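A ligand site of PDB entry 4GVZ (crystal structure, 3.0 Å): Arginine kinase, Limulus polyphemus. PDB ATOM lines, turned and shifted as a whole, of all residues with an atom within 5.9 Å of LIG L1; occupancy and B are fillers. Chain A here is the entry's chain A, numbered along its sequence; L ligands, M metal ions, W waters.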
ATOM      1  N   SER A  56      10.624  12.585  -8.234  1.00  0.00           N
ATOM      2  CA  SER A  56      10.595  11.151  -7.995  1.00  0.00           C
ATOM      3  C   SER A  56       9.444  10.509  -8.761  1.00  0.00           C
ATOM      4  O   SER A  56       9.557   9.394  -9.268  1.00  0.00           O
ATOM      5  CB  SER A  56      10.409  10.860  -6.501  1.00  0.00           C
ATOM      6  OG  SER A  56      10.330   9.466  -6.255  1.00  0.00           O
ATOM      7  N   ASP A  62       5.443   4.418 -12.061  1.00  0.00           N
ATOM      8  CA  ASP A  62       4.658   3.424 -11.332  1.00  0.00           C
ATOM      9  C   ASP A  62       4.344   3.859  -9.902  1.00  0.00           C
ATOM     10  O   ASP A  62       3.697   3.134  -9.149  1.00  0.00           O
ATOM     11  CB  ASP A  62       5.370   2.072 -11.316  1.00  0.00           C
ATOM     12  CG  ASP A  62       6.745   2.143 -10.668  1.00  0.00           C
ATOM     13  OD1 ASP A  62       7.346   3.239 -10.648  1.00  0.00           O
ATOM     14  OD2 ASP A  62       7.220   1.093 -10.177  1.00  0.00           O
ATOM     15  N   SER A  63       4.797   5.060  -9.535  1.00  0.00           N
ATOM     16  CA  SER A  63       4.522   5.625  -8.224  1.00  0.00           C
ATOM     17  C   SER A  63       3.021   5.614  -7.906  1.00  0.00           C
ATOM     18  O   SER A  63       2.187   5.779  -8.803  1.00  0.00           O
ATOM     19  CB  SER A  63       5.046   7.053  -8.125  1.00  0.00           C
ATOM     20  OG  SER A  63       6.458   7.070  -8.200  1.00  0.00           O
ATOM     21  N   GLY A  64       2.690   5.400  -6.643  1.00  0.00           N
ATOM     22  CA  GLY A  64       1.330   5.586  -6.168  1.00  0.00           C
ATOM     23  C   GLY A  64       1.050   7.036  -5.805  1.00  0.00           C
ATOM     24  O   GLY A  64      -0.074   7.512  -5.963  1.00  0.00           O
ATOM     25  N   VAL A  65       2.082   7.742  -5.341  1.00  0.00           N
ATOM     26  CA  VAL A  65       1.932   9.129  -4.896  1.00  0.00           C
ATOM     27  C   VAL A  65       2.784  10.059  -5.749  1.00  0.00           C
ATOM     28  O   VAL A  65       2.265  10.914  -6.457  1.00  0.00           O
ATOM     29  CB  VAL A  65       2.296   9.283  -3.410  1.00  0.00           C
ATOM     30  CG1 VAL A  65       2.107  10.721  -2.962  1.00  0.00           C
ATOM     31  CG2 VAL A  65       1.456   8.344  -2.565  1.00  0.00           C
ATOM     32  N   GLY A  66       4.101   9.894  -5.659  1.00  0.00           N
ATOM     33  CA  GLY A  66       5.005  10.545  -6.597  1.00  0.00           C
ATOM     34  C   GLY A  66       5.660  11.836  -6.146  1.00  0.00           C
ATOM     35  O   GLY A  66       6.425  12.428  -6.910  1.00  0.00           O
ATOM     36  N   ILE A  67       5.388  12.279  -4.926  1.00  0.00           N
ATOM     37  CA  ILE A  67       5.970  13.522  -4.441  1.00  0.00           C
ATOM     38  C   ILE A  67       6.563  13.425  -3.040  1.00  0.00           C
ATOM     39  O   ILE A  67       6.176  12.575  -2.248  1.00  0.00           O
ATOM     40  CB  ILE A  67       4.942  14.671  -4.449  1.00  0.00           C
ATOM     41  CG1 ILE A  67       3.817  14.381  -3.463  1.00  0.00           C
ATOM     42  CG2 ILE A  67       4.412  14.892  -5.858  1.00  0.00           C
ATOM     43  CD1 ILE A  67       2.864  15.542  -3.268  1.00  0.00           C
ATOM     44  N   TYR A  68       7.509  14.320  -2.755  1.00  0.00           N
ATOM     45  CA  TYR A  68       8.092  14.425  -1.425  1.00  0.00           C
ATOM     46  C   TYR A  68       8.326  15.895  -1.094  1.00  0.00           C
ATOM     47  O   TYR A  68       8.376  16.744  -1.983  1.00  0.00           O
ATOM     48  CB  TYR A  68       9.447  13.729  -1.396  1.00  0.00           C
ATOM     49  CG  TYR A  68       9.390  12.220  -1.531  1.00  0.00           C
ATOM     50  CD1 TYR A  68       9.515  11.622  -2.783  1.00  0.00           C
ATOM     51  CD2 TYR A  68       9.229  11.414  -0.427  1.00  0.00           C
ATOM     52  CE1 TYR A  68       9.457  10.247  -2.919  1.00  0.00           C
ATOM     53  CE2 TYR A  68       9.179  10.036  -0.551  1.00  0.00           C
ATOM     54  CZ  TYR A  68       9.292   9.456  -1.792  1.00  0.00           C
ATOM     55  OH  TYR A  68       9.254   8.089  -1.921  1.00  0.00           O
ATOM     56  N   ARG A 126       4.565   1.220  13.527  1.00  0.00           N
ATOM     57  CA  ARG A 126       5.621   2.233  13.476  1.00  0.00           C
ATOM     58  C   ARG A 126       5.114   3.676  13.451  1.00  0.00           C
ATOM     59  O   ARG A 126       3.992   3.943  13.011  1.00  0.00           O
ATOM     60  CB  ARG A 126       6.582   1.950  12.314  1.00  0.00           C
ATOM     61  CG  ARG A 126       5.972   2.041  10.938  1.00  0.00           C
ATOM     62  CD  ARG A 126       5.870   3.469  10.431  1.00  0.00           C
ATOM     63  NE  ARG A 126       5.555   3.494   9.010  1.00  0.00           N
ATOM     64  CZ  ARG A 126       5.021   4.529   8.373  1.00  0.00           C
ATOM     65  NH1 ARG A 126       4.785   4.453   7.065  1.00  0.00           N
ATOM     66  NH2 ARG A 126       4.682   5.619   9.038  1.00  0.00           N
ATOM     67  N   ASP A 192      16.164   2.075  -2.675  1.00  0.00           N
ATOM     68  CA  ASP A 192      14.794   2.296  -3.084  1.00  0.00           C
ATOM     69  C   ASP A 192      14.806   3.368  -4.175  1.00  0.00           C
ATOM     70  O   ASP A 192      15.214   4.499  -3.942  1.00  0.00           O
ATOM     71  CB  ASP A 192      13.944   2.768  -1.901  1.00  0.00           C
ATOM     72  CG  ASP A 192      12.525   3.117  -2.282  1.00  0.00           C
ATOM     73  OD1 ASP A 192      12.336   3.996  -3.152  1.00  0.00           O
ATOM     74  OD2 ASP A 192      11.593   2.515  -1.722  1.00  0.00           O
ATOM     75  N   PHE A 194      12.527   5.066  -5.627  1.00  0.00           N
ATOM     76  CA  PHE A 194      11.675   6.232  -5.415  1.00  0.00           C
ATOM     77  C   PHE A 194      12.368   7.252  -4.520  1.00  0.00           C
ATOM     78  O   PHE A 194      12.292   8.455  -4.777  1.00  0.00           O
ATOM     79  CB  PHE A 194      10.362   5.799  -4.766  1.00  0.00           C
ATOM     80  CG  PHE A 194       9.590   4.776  -5.555  1.00  0.00           C
ATOM     81  CD1 PHE A 194       9.721   3.430  -5.264  1.00  0.00           C
ATOM     82  CD2 PHE A 194       8.741   5.156  -6.575  1.00  0.00           C
ATOM     83  CE1 PHE A 194       9.021   2.482  -5.986  1.00  0.00           C
ATOM     84  CE2 PHE A 194       8.034   4.220  -7.306  1.00  0.00           C
ATOM     85  CZ  PHE A 194       8.172   2.871  -7.004  1.00  0.00           C
ATOM     86  N   LEU A 195      13.042   6.768  -3.485  1.00  0.00           N
ATOM     87  CA  LEU A 195      13.772   7.639  -2.573  1.00  0.00           C
ATOM     88  C   LEU A 195      15.034   8.207  -3.225  1.00  0.00           C
ATOM     89  O   LEU A 195      15.365   9.382  -3.044  1.00  0.00           O
ATOM     90  CB  LEU A 195      14.151   6.887  -1.295  1.00  0.00           C
ATOM     91  CG  LEU A 195      12.999   6.640  -0.316  1.00  0.00           C
ATOM     92  CD1 LEU A 195      13.396   5.674   0.778  1.00  0.00           C
ATOM     93  CD2 LEU A 195      12.501   7.959   0.266  1.00  0.00           C
ATOM     94  N   GLU A 225      14.262   7.070   5.259  1.00  0.00           N
ATOM     95  CA  GLU A 225      13.317   7.986   4.625  1.00  0.00           C
ATOM     96  C   GLU A 225      13.028   9.181   5.540  1.00  0.00           C
ATOM     97  O   GLU A 225      12.943  10.319   5.086  1.00  0.00           O
ATOM     98  CB  GLU A 225      12.008   7.267   4.277  1.00  0.00           C
ATOM     99  CG  GLU A 225      10.939   8.196   3.731  1.00  0.00           C
ATOM    100  CD  GLU A 225       9.697   7.452   3.267  1.00  0.00           C
ATOM    101  OE1 GLU A 225       8.603   8.061   3.285  1.00  0.00           O
ATOM    102  OE2 GLU A 225       9.826   6.276   2.887  1.00  0.00           O
ATOM    103  N   ARG A 229      12.461   6.474  12.533  1.00  0.00           N
ATOM    104  CA  ARG A 229      11.269   5.643  12.560  1.00  0.00           C
ATOM    105  C   ARG A 229      11.281   4.833  13.845  1.00  0.00           C
ATOM    106  O   ARG A 229      12.271   4.177  14.160  1.00  0.00           O
ATOM    107  CB  ARG A 229      11.250   4.684  11.366  1.00  0.00           C
ATOM    108  CG  ARG A 229      11.057   5.357  10.023  1.00  0.00           C
ATOM    109  CD  ARG A 229       9.644   5.904   9.891  1.00  0.00           C
ATOM    110  NE  ARG A 229       9.355   6.404   8.546  1.00  0.00           N
ATOM    111  CZ  ARG A 229       9.152   5.622   7.484  1.00  0.00           C
ATOM    112  NH1 ARG A 229       9.188   4.304   7.619  1.00  0.00           N
ATOM    113  NH2 ARG A 229       8.921   6.155   6.299  1.00  0.00           N
ATOM    114  N   CYS A 271       7.582  12.101   3.354  1.00  0.00           N
ATOM    115  CA  CYS A 271       6.485  11.833   2.435  1.00  0.00           C
ATOM    116  C   CYS A 271       5.176  12.315   3.046  1.00  0.00           C
ATOM    117  O   CYS A 271       4.945  12.145   4.249  1.00  0.00           O
ATOM    118  CB  CYS A 271       6.413  10.339   2.109  1.00  0.00           C
ATOM    119  SG  CYS A 271       5.056   9.871   1.012  1.00  0.00           S
ATOM    120  N   THR A 273       2.311  11.055   2.740  1.00  0.00           N
ATOM    121  CA  THR A 273       1.497   9.918   3.163  1.00  0.00           C
ATOM    122  C   THR A 273       1.703   9.592   4.644  1.00  0.00           C
ATOM    123  O   THR A 273       0.907   8.885   5.247  1.00  0.00           O
ATOM    124  CB  THR A 273       1.845   8.653   2.364  1.00  0.00           C
ATOM    125  OG1 THR A 273       3.213   8.285   2.610  1.00  0.00           O
ATOM    126  CG2 THR A 273       1.633   8.887   0.880  1.00  0.00           C
ATOM    127  N   ASN A 274       2.782  10.130   5.208  1.00  0.00           N
ATOM    128  CA  ASN A 274       3.179   9.797   6.578  1.00  0.00           C
ATOM    129  C   ASN A 274       2.902  10.897   7.590  1.00  0.00           C
ATOM    130  O   ASN A 274       3.320  10.812   8.738  1.00  0.00           O
ATOM    131  CB  ASN A 274       4.655   9.384   6.620  1.00  0.00           C
ATOM    132  CG  ASN A 274       4.888   7.985   6.087  1.00  0.00           C
ATOM    133  OD1 ASN A 274       4.130   7.063   6.384  1.00  0.00           O
ATOM    134  ND2 ASN A 274       5.927   7.822   5.280  1.00  0.00           N
ATOM    135  N   ARG A 309       0.434  -4.579   1.163  1.00  0.00           N
ATOM    136  CA  ARG A 309       1.821  -4.567   0.720  1.00  0.00           C
ATOM    137  C   ARG A 309       2.352  -5.998   0.692  1.00  0.00           C
ATOM    138  O   ARG A 309       1.747  -6.904   1.255  1.00  0.00           O
ATOM    139  CB  ARG A 309       2.672  -3.729   1.677  1.00  0.00           C
ATOM    140  CG  ARG A 309       2.299  -2.249   1.663  1.00  0.00           C
ATOM    141  CD  ARG A 309       3.089  -1.458   2.688  1.00  0.00           C
ATOM    142  NE  ARG A 309       2.722  -0.049   2.669  1.00  0.00           N
ATOM    143  CZ  ARG A 309       3.531   0.950   2.996  1.00  0.00           C
ATOM    144  NH1 ARG A 309       4.787   0.700   3.358  1.00  0.00           N
ATOM    145  NH2 ARG A 309       3.109   2.202   2.947  1.00  0.00           N
ATOM    146  N   GLU A 314       6.435  -2.455   0.958  1.00  0.00           N
ATOM    147  CA  GLU A 314       5.850  -1.871  -0.243  1.00  0.00           C
ATOM    148  C   GLU A 314       6.650  -2.225  -1.485  1.00  0.00           C
ATOM    149  O   GLU A 314       7.858  -2.433  -1.422  1.00  0.00           O
ATOM    150  CB  GLU A 314       5.718  -0.353  -0.090  1.00  0.00           C
ATOM    151  CG  GLU A 314       7.028   0.366   0.216  1.00  0.00           C
ATOM    152  CD  GLU A 314       6.914   1.872   0.116  1.00  0.00           C
ATOM    153  OE1 GLU A 314       5.789   2.376  -0.068  1.00  0.00           O
ATOM    154  OE2 GLU A 314       7.953   2.554   0.206  1.00  0.00           O
ATOM    155  N   HIS A 315       5.961  -2.302  -2.624  1.00  0.00           N
ATOM    156  CA  HIS A 315       6.595  -2.549  -3.916  1.00  0.00           C
ATOM    157  C   HIS A 315       7.197  -3.954  -4.015  1.00  0.00           C
ATOM    158  O   HIS A 315       8.090  -4.193  -4.836  1.00  0.00           O
ATOM    159  CB  HIS A 315       7.678  -1.502  -4.195  1.00  0.00           C
ATOM    160  CG  HIS A 315       7.224  -0.096  -3.983  1.00  0.00           C
ATOM    161  ND1 HIS A 315       7.874   0.769  -3.125  1.00  0.00           N
ATOM    162  CD2 HIS A 315       6.198   0.603  -4.519  1.00  0.00           C
ATOM    163  CE1 HIS A 315       7.254   1.946  -3.147  1.00  0.00           C
ATOM    164  NE2 HIS A 315       6.243   1.862  -3.980  1.00  0.00           N
HETATM  165  N1  LIG L   1       7.452   7.184  -3.870  1.00  0.00           N
HETATM  166  C1  LIG L   1       6.054   7.124  -3.441  1.00  0.00           C
HETATM  167  C2  LIG L   1       6.015   6.622  -1.980  1.00  0.00           C
HETATM  168  C3  LIG L   1       4.633   6.116  -1.535  1.00  0.00           C
HETATM  169  C4  LIG L   1       4.573   6.151   0.004  1.00  0.00           C
HETATM  170  N2  LIG L   1       5.626   5.333   0.604  1.00  0.00           N
HETATM  171  C5  LIG L   1       6.582   5.845   1.501  1.00  0.00           C
HETATM  172  N3  LIG L   1       6.484   7.213   1.807  1.00  0.00           N
HETATM  173  N4  LIG L   1       7.557   5.176   2.084  1.00  0.00           N
HETATM  174  C6  LIG L   1       5.264   6.130  -4.355  1.00  0.00           C
HETATM  175  O1  LIG L   1       4.492   6.649  -5.185  1.00  0.00           O
HETATM  176  O2  LIG L   1       5.471   4.912  -4.216  1.00  0.00           O
HETATM  177  P1  LG2 L   2       7.424   1.318   6.759  1.00  0.00           P
HETATM  178  O1  LG2 L   2       8.097   2.276   5.802  1.00  0.00           O
HETATM  179  O2  LG2 L   2       8.261   0.696   7.847  1.00  0.00           O
HETATM  180  O3  LG2 L   2       6.030   1.788   7.123  1.00  0.00           O
HETATM  181  P2  LG2 L   2       7.714  -0.731   4.553  1.00  0.00           P
HETATM  182  O4  LG2 L   2       8.729   0.062   3.794  1.00  0.00           O
HETATM  183  O5  LG2 L   2       6.806  -1.697   3.837  1.00  0.00           O
HETATM  184  O6  LG2 L   2       7.292  -0.290   5.967  1.00  0.00           O
HETATM  185  O7  LG2 L   2       8.920  -2.080   5.004  1.00  0.00           O
HETATM  186  C1  LG2 L   2       9.706  -2.030   6.078  1.00  0.00           C
HETATM  187  C2  LG2 L   2      10.022  -3.493   6.632  1.00  0.00           C
HETATM  188  O8  LG2 L   2       9.062  -3.841   7.637  1.00  0.00           O
HETATM  189  C3  LG2 L   2       9.906  -4.588   5.540  1.00  0.00           C
HETATM  190  O9  LG2 L   2      11.006  -5.460   5.504  1.00  0.00           O
HETATM  191  C4  LG2 L   2       8.693  -5.467   5.984  1.00  0.00           C
HETATM  192  O10 LG2 L   2       9.024  -6.822   5.911  1.00  0.00           O
HETATM  193  C5  LG2 L   2       8.623  -5.135   7.484  1.00  0.00           C
HETATM  194  N1  LG2 L   2       7.241  -5.295   8.074  1.00  0.00           N
HETATM  195  C6  LG2 L   2       6.168  -4.379   7.884  1.00  0.00           C
HETATM  196  N2  LG2 L   2       5.038  -4.760   8.519  1.00  0.00           N
HETATM  197  C7  LG2 L   2       5.384  -5.965   9.153  1.00  0.00           C
HETATM  198  C8  LG2 L   2       4.647  -6.848   9.973  1.00  0.00           C
HETATM  199  N3  LG2 L   2       3.322  -6.603  10.281  1.00  0.00           N
HETATM  200  N4  LG2 L   2       5.222  -7.988  10.490  1.00  0.00           N
HETATM  201  C9  LG2 L   2       6.538  -8.185  10.149  1.00  0.00           C
HETATM  202  N5  LG2 L   2       7.356  -7.438   9.381  1.00  0.00           N
HETATM  203  C10 LG2 L   2       6.744  -6.303   8.885  1.00  0.00           C
HETATM  204 MG    MG M   1       9.340   2.097   4.016  1.00  0.00          MG
HETATM  205  O   HOH W   1       7.773   8.631  -6.424  1.00  0.00           O
HETATM  206  O   HOH W   2       9.852   6.197   0.026  1.00  0.00           O
HETATM  207  O   HOH W   3       5.406  10.021  -2.442  1.00  0.00           O
HETATM  208  O   HOH W   4       2.201   4.848   1.871  1.00  0.00           O
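The side-chain hydroxyl (OH) of Tyr 68 lies within hydrogen-bond range of a nitrogen (N1) of LIG L1, 2.8 Å away.
NH1 of Arg 309 is in salt-bridge range of O5 of LG2 L2 (3.2 Å).
A nitrogen (N2) of LIG L1 is in salt-bridge range of the side-chain carboxylate (OE1) of Glu 314.
The side-chain carboxylate (OE2) of Glu 225 lies within salt-bridge range of a nitrogen (N4) of LIG L1 (2.6 Å).
N of Glu 314 lies within hydrogen-bond range of O5 of LG2 L2 (3.0 Å).
The backbone NH (N) of Gly 64 sits at hydrogen-bond distance from an oxygen (O1) of LIG L1 (2.6 Å).
O2 of LIG L1 sits at hydrogen-bond distance from NE2 of His 315 (3.2 Å).
An oxygen (O1) of LIG L1 sits at hydrogen-bond distance from the backbone NH of Gly 66 (3.3 Å).
A nitrogen (N3) of LIG L1 is in hydrogen-bond range of the side-chain sulfur of Cys 271 (3.1 Å).
An oxygen (O3) of LG2 L2 lies within salt-bridge range of the guanidinium group (NE) of Arg 126, 2.6 Å away.
An oxygen (O1) of LIG L1 lies within hydrogen-bond range of the backbone NH (N) of Val 65, 2.7 Å away.
NH1 of Arg 229 lies within salt-bridge range of O2 of LG2 L2.
O of Phe 194 is in hydrogen-bond range of OG of Ser 56 (2.7 Å).
The side-chain amide oxygen of Asn 274 lies within hydrogen-bond range of the guanidinium group of Arg 126 (2.8 Å).
OE1 of Glu 225 lies within hydrogen-bond range of ND2 of Asn 274 (3.3 Å).
The backbone NH of Phe 194 sits at hydrogen-bond distance from the side-chain carboxylate of Asp 192.
The side-chain carboxylate (OE1) of Glu 314 lies within salt-bridge range of the guanidinium group (NH1) of Arg 309 (3.9 Å).
The guanidinium group of Arg 229 lies within salt-bridge range of the side-chain carboxylate of Glu 225.
The side-chain sulfur of Cys 271 is in hydrogen-bond range of the side-chain hydroxyl of Thr 273 (2.9 Å).
Ser 63 touches LIG L1.
Phe 194 touches LIG L1.
OG1 of Thr 273 touches N3 of LIG L1 (3.5 Å).
Asn 274 touches LIG L1.
Hydrophobic or aromatic side chains that line LIG L1: Val 65, Tyr 68, Phe 194 and His 315.
12 residues have an atom within 4 Å of LIG L1: Ser 63, Gly 64, Val 65, Gly 66, Tyr 68, Phe 194, Glu 225, Cys 271, Thr 273, Asn 274, Glu 314 and His 315.
The nearest printed residue that does not touch LIG L1 is Ser 56 (4.4 Å).
Water W1 lies within hydrogen-bond range of OG of Ser 56, OG of Ser 63 and N1 of LIG L1.
Water W3 lies within hydrogen-bond range of the backbone carbonyl oxygen (O) of Ile 67 (2.7 Å), the backbone NH (N) of Gly 66 (3.5 Å) and the side-chain sulfur (SG) of Cys 271 (3.5 Å).
Water W2 lies within hydrogen-bond range of the side-chain hydroxyl (OH) of Tyr 68, the side-chain carboxylate (OE2) of Glu 225 and a nitrogen (N4) of LIG L1.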
